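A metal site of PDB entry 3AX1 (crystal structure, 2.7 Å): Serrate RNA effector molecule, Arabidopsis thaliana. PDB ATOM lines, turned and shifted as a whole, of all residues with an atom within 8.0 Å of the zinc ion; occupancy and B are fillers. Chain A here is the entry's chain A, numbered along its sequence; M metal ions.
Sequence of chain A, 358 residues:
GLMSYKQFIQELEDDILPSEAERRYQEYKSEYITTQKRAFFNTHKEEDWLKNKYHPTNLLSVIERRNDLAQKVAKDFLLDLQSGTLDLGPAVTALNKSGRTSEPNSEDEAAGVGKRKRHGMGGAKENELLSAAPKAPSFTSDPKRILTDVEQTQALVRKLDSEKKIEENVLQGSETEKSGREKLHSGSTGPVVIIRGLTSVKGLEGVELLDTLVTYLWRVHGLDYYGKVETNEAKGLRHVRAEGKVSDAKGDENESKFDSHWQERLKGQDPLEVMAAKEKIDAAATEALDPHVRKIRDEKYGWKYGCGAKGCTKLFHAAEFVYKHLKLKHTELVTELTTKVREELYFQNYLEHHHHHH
The backbone NH (N) of Lys 314 lies close to the side-chain sulfur (SG) of Cys 312 (3.7 Å). O of Cys 312 lies within hydrogen-bond range of NH2 of Arg 294 (3.3 Å). The side-chain sulfur (SG) of Cys 307 lies close to the backbone NH (N) of Ala 309 (3.5 Å). The backbone NH (N) of Cys 307 lies within hydrogen-bond range of the backbone carbonyl oxygen (O) of Lys 314. O of Cys 307 sits at hydrogen-bond distance from NH2 of Arg 294 (2.6 Å).
The zinc ion is bound by NE2 of His 325 (2.2 Å), SG of Cys 312 (2.3 Å), NE2 of His 330 (2.4 Å) and SG of Cys 307 (2.5 Å).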
ATOM      1  N   HIS A 292       5.700  20.199  11.061  1.00  0.00           N
ATOM      2  CA  HIS A 292       5.127  20.742   9.849  1.00  0.00           C
ATOM      3  C   HIS A 292       6.141  21.123   8.797  1.00  0.00           C
ATOM      4  O   HIS A 292       5.802  21.875   7.886  1.00  0.00           O
ATOM      5  CB  HIS A 292       4.282  21.974  10.189  1.00  0.00           C
ATOM      6  CG  HIS A 292       3.043  21.649  10.943  1.00  0.00           C
ATOM      7  ND1 HIS A 292       1.872  21.258  10.317  1.00  0.00           N
ATOM      8  CD2 HIS A 292       2.783  21.634  12.268  1.00  0.00           C
ATOM      9  CE1 HIS A 292       0.946  21.033  11.221  1.00  0.00           C
ATOM     10  NE2 HIS A 292       1.468  21.250  12.419  1.00  0.00           N
ATOM     11  N   ARG A 294       8.561  19.129   6.151  1.00  0.00           N
ATOM     12  CA  ARG A 294       9.040  17.875   5.535  1.00  0.00           C
ATOM     13  C   ARG A 294      10.490  18.018   5.066  1.00  0.00           C
ATOM     14  O   ARG A 294      10.810  18.847   4.228  1.00  0.00           O
ATOM     15  CB  ARG A 294       8.160  17.425   4.344  1.00  0.00           C
ATOM     16  CG  ARG A 294       6.668  17.846   4.383  1.00  0.00           C
ATOM     17  CD  ARG A 294       6.008  17.841   2.966  1.00  0.00           C
ATOM     18  NE  ARG A 294       4.883  18.797   2.835  1.00  0.00           N
ATOM     19  CZ  ARG A 294       3.569  18.468   2.871  1.00  0.00           C
ATOM     20  NH1 ARG A 294       3.172  17.217   3.049  1.00  0.00           N
ATOM     21  NH2 ARG A 294       2.637  19.428   2.733  1.00  0.00           N
ATOM     22  N   GLY A 306      10.165  21.029   2.579  1.00  0.00           N
ATOM     23  CA  GLY A 306       8.832  21.266   2.063  1.00  0.00           C
ATOM     24  C   GLY A 306       7.858  21.603   3.171  1.00  0.00           C
ATOM     25  O   GLY A 306       7.946  21.061   4.272  1.00  0.00           O
ATOM     26  N   CYS A 307       6.921  22.499   2.862  1.00  0.00           N
ATOM     27  CA  CYS A 307       5.954  22.955   3.848  1.00  0.00           C
ATOM     28  C   CYS A 307       4.869  21.930   4.085  1.00  0.00           C
ATOM     29  O   CYS A 307       4.251  21.465   3.125  1.00  0.00           O
ATOM     30  CB  CYS A 307       5.314  24.268   3.408  1.00  0.00           C
ATOM     31  SG  CYS A 307       3.849  24.646   4.374  1.00  0.00           S
ATOM     32  N   GLY A 308       4.630  21.601   5.351  1.00  0.00           N
ATOM     33  CA  GLY A 308       3.715  20.523   5.754  1.00  0.00           C
ATOM     34  C   GLY A 308       2.295  20.916   6.165  1.00  0.00           C
ATOM     35  O   GLY A 308       1.567  20.113   6.757  1.00  0.00           O
ATOM     36  N   ALA A 309       1.899  22.155   5.877  1.00  0.00           N
ATOM     37  CA  ALA A 309       0.515  22.571   6.054  1.00  0.00           C
ATOM     38  C   ALA A 309      -0.275  21.952   4.911  1.00  0.00           C
ATOM     39  O   ALA A 309       0.312  21.397   3.955  1.00  0.00           O
ATOM     40  CB  ALA A 309       0.406  24.078   6.031  1.00  0.00           C
ATOM     41  N   LYS A 310      -1.608  22.039   4.997  1.00  0.00           N
ATOM     42  CA  LYS A 310      -2.493  21.408   3.998  1.00  0.00           C
ATOM     43  C   LYS A 310      -2.909  22.328   2.869  1.00  0.00           C
ATOM     44  O   LYS A 310      -3.054  23.547   3.040  1.00  0.00           O
ATOM     45  CB  LYS A 310      -3.687  20.714   4.649  1.00  0.00           C
ATOM     46  CG  LYS A 310      -3.290  19.407   5.327  1.00  0.00           C
ATOM     47  CD  LYS A 310      -4.375  18.859   6.262  1.00  0.00           C
ATOM     48  CE  LYS A 310      -3.710  18.121   7.426  1.00  0.00           C
ATOM     49  NZ  LYS A 310      -4.370  16.795   7.705  1.00  0.00           N
ATOM     50  N   GLY A 311      -3.083  21.711   1.697  1.00  0.00           N
ATOM     51  CA  GLY A 311      -3.361  22.454   0.470  1.00  0.00           C
ATOM     52  C   GLY A 311      -2.069  22.989  -0.125  1.00  0.00           C
ATOM     53  O   GLY A 311      -2.045  23.416  -1.286  1.00  0.00           O
ATOM     54  N   CYS A 312      -0.994  22.924   0.670  1.00  0.00           N
ATOM     55  CA  CYS A 312       0.260  23.593   0.335  1.00  0.00           C
ATOM     56  C   CYS A 312       1.392  22.668  -0.150  1.00  0.00           C
ATOM     57  O   CYS A 312       1.629  21.596   0.412  1.00  0.00           O
ATOM     58  CB  CYS A 312       0.733  24.431   1.515  1.00  0.00           C
ATOM     59  SG  CYS A 312       2.153  25.384   1.066  1.00  0.00           S
ATOM     60  N   THR A 313       2.086  23.117  -1.197  1.00  0.00           N
ATOM     61  CA  THR A 313       3.066  22.306  -1.913  1.00  0.00           C
ATOM     62  C   THR A 313       4.410  23.016  -2.111  1.00  0.00           C
ATOM     63  O   THR A 313       5.289  22.502  -2.816  1.00  0.00           O
ATOM     64  CB  THR A 313       2.563  21.917  -3.324  1.00  0.00           C
ATOM     65  OG1 THR A 313       1.126  21.944  -3.341  1.00  0.00           O
ATOM     66  CG2 THR A 313       3.053  20.525  -3.735  1.00  0.00           C
ATOM     67  N   LYS A 314       4.567  24.194  -1.499  1.00  0.00           N
ATOM     68  CA  LYS A 314       5.782  25.007  -1.708  1.00  0.00           C
ATOM     69  C   LYS A 314       7.053  24.341  -1.170  1.00  0.00           C
ATOM     70  O   LYS A 314       7.013  23.640  -0.148  1.00  0.00           O
ATOM     71  CB  LYS A 314       5.616  26.451  -1.210  1.00  0.00           C
ATOM     72  CG  LYS A 314       4.739  27.304  -2.167  1.00  0.00           C
ATOM     73  CD  LYS A 314       4.649  28.775  -1.740  1.00  0.00           C
ATOM     74  CE  LYS A 314       3.248  29.382  -2.010  1.00  0.00           C
ATOM     75  NZ  LYS A 314       2.808  30.394  -0.968  1.00  0.00           N
ATOM     76  N   LEU A 315       8.170  24.540  -1.870  1.00  0.00           N
ATOM     77  CA  LEU A 315       9.455  23.951  -1.522  1.00  0.00           C
ATOM     78  C   LEU A 315      10.529  25.015  -1.334  1.00  0.00           C
ATOM     79  O   LEU A 315      10.621  25.953  -2.130  1.00  0.00           O
ATOM     80  CB  LEU A 315       9.906  22.964  -2.603  1.00  0.00           C
ATOM     81  CG  LEU A 315       8.930  21.851  -2.994  1.00  0.00           C
ATOM     82  CD1 LEU A 315       9.322  21.230  -4.343  1.00  0.00           C
ATOM     83  CD2 LEU A 315       8.795  20.800  -1.888  1.00  0.00           C
ATOM     84  N   PHE A 316      11.349  24.853  -0.306  1.00  0.00           N
ATOM     85  CA  PHE A 316      12.363  25.821   0.073  1.00  0.00           C
ATOM     86  C   PHE A 316      13.710  25.143   0.187  1.00  0.00           C
ATOM     87  O   PHE A 316      13.766  23.923   0.203  1.00  0.00           O
ATOM     88  CB  PHE A 316      12.002  26.448   1.414  1.00  0.00           C
ATOM     89  CG  PHE A 316      10.670  27.141   1.409  1.00  0.00           C
ATOM     90  CD1 PHE A 316       9.497  26.410   1.598  1.00  0.00           C
ATOM     91  CD2 PHE A 316      10.585  28.514   1.197  1.00  0.00           C
ATOM     92  CE1 PHE A 316       8.279  27.035   1.587  1.00  0.00           C
ATOM     93  CE2 PHE A 316       9.368  29.163   1.182  1.00  0.00           C
ATOM     94  CZ  PHE A 316       8.199  28.424   1.378  1.00  0.00           C
ATOM     95  N   VAL A 322      11.108  27.837   5.509  1.00  0.00           N
ATOM     96  CA  VAL A 322       9.772  27.289   5.783  1.00  0.00           C
ATOM     97  C   VAL A 322       9.124  27.879   7.038  1.00  0.00           C
ATOM     98  O   VAL A 322       7.939  28.187   7.024  1.00  0.00           O
ATOM     99  CB  VAL A 322       9.769  25.762   5.901  1.00  0.00           C
ATOM    100  CG1 VAL A 322       8.357  25.254   5.869  1.00  0.00           C
ATOM    101  CG2 VAL A 322      10.560  25.137   4.765  1.00  0.00           C
ATOM    102  N   HIS A 325       7.939  31.220   6.181  1.00  0.00           N
ATOM    103  CA  HIS A 325       6.776  31.082   5.301  1.00  0.00           C
ATOM    104  C   HIS A 325       5.492  30.760   6.063  1.00  0.00           C
ATOM    105  O   HIS A 325       4.432  31.327   5.762  1.00  0.00           O
ATOM    106  CB  HIS A 325       7.034  30.037   4.226  1.00  0.00           C
ATOM    107  CG  HIS A 325       5.783  29.417   3.691  1.00  0.00           C
ATOM    108  ND1 HIS A 325       4.926  30.086   2.846  1.00  0.00           N
ATOM    109  CD2 HIS A 325       5.243  28.197   3.892  1.00  0.00           C
ATOM    110  CE1 HIS A 325       3.914  29.295   2.531  1.00  0.00           C
ATOM    111  NE2 HIS A 325       4.077  28.138   3.157  1.00  0.00           N
ATOM    112  N   LEU A 326       5.603  29.850   7.041  1.00  0.00           N
ATOM    113  CA  LEU A 326       4.488  29.432   7.886  1.00  0.00           C
ATOM    114  C   LEU A 326       3.832  30.586   8.645  1.00  0.00           C
ATOM    115  O   LEU A 326       2.613  30.712   8.624  1.00  0.00           O
ATOM    116  CB  LEU A 326       4.902  28.311   8.842  1.00  0.00           C
ATOM    117  CG  LEU A 326       4.963  26.918   8.211  1.00  0.00           C
ATOM    118  CD1 LEU A 326       5.966  26.029   8.903  1.00  0.00           C
ATOM    119  CD2 LEU A 326       3.585  26.246   8.193  1.00  0.00           C
ATOM    120  N   LYS A 329       1.940  32.714   5.752  1.00  0.00           N
ATOM    121  CA  LYS A 329       0.951  32.150   4.850  1.00  0.00           C
ATOM    122  C   LYS A 329       0.040  31.182   5.594  1.00  0.00           C
ATOM    123  O   LYS A 329      -0.924  30.655   5.016  1.00  0.00           O
ATOM    124  CB  LYS A 329       1.636  31.466   3.661  1.00  0.00           C
ATOM    125  CG  LYS A 329       2.305  32.425   2.697  1.00  0.00           C
ATOM    126  CD  LYS A 329       1.503  32.576   1.404  1.00  0.00           C
ATOM    127  CE  LYS A 329       1.834  33.876   0.649  1.00  0.00           C
ATOM    128  NZ  LYS A 329       3.285  34.215   0.624  1.00  0.00           N
ATOM    129  N   HIS A 330       0.360  30.966   6.875  1.00  0.00           N
ATOM    130  CA  HIS A 330      -0.424  30.109   7.755  1.00  0.00           C
ATOM    131  C   HIS A 330      -0.448  30.673   9.170  1.00  0.00           C
ATOM    132  O   HIS A 330      -0.254  29.931  10.129  1.00  0.00           O
ATOM    133  CB  HIS A 330       0.121  28.698   7.767  1.00  0.00           C
ATOM    134  CG  HIS A 330       0.333  28.120   6.408  1.00  0.00           C
ATOM    135  ND1 HIS A 330      -0.707  27.813   5.561  1.00  0.00           N
ATOM    136  CD2 HIS A 330       1.465  27.781   5.744  1.00  0.00           C
ATOM    137  CE1 HIS A 330      -0.231  27.319   4.437  1.00  0.00           C
ATOM    138  NE2 HIS A 330       1.086  27.296   4.516  1.00  0.00           N
ATOM    139  N   LEU A 333      -2.588  28.735  12.007  1.00  0.00           N
ATOM    140  CA  LEU A 333      -1.956  27.446  12.352  1.00  0.00           C
ATOM    141  C   LEU A 333      -0.773  27.666  13.255  1.00  0.00           C
ATOM    142  O   LEU A 333      -0.525  26.849  14.132  1.00  0.00           O
ATOM    143  CB  LEU A 333      -1.505  26.648  11.122  1.00  0.00           C
ATOM    144  CG  LEU A 333      -0.599  25.407  11.327  1.00  0.00           C
ATOM    145  CD1 LEU A 333      -1.224  24.267  12.168  1.00  0.00           C
ATOM    146  CD2 LEU A 333      -0.098  24.835  10.001  1.00  0.00           C
HETATM  147 ZN    ZN M   1       2.742  26.440   3.052  1.00  0.00          ZN
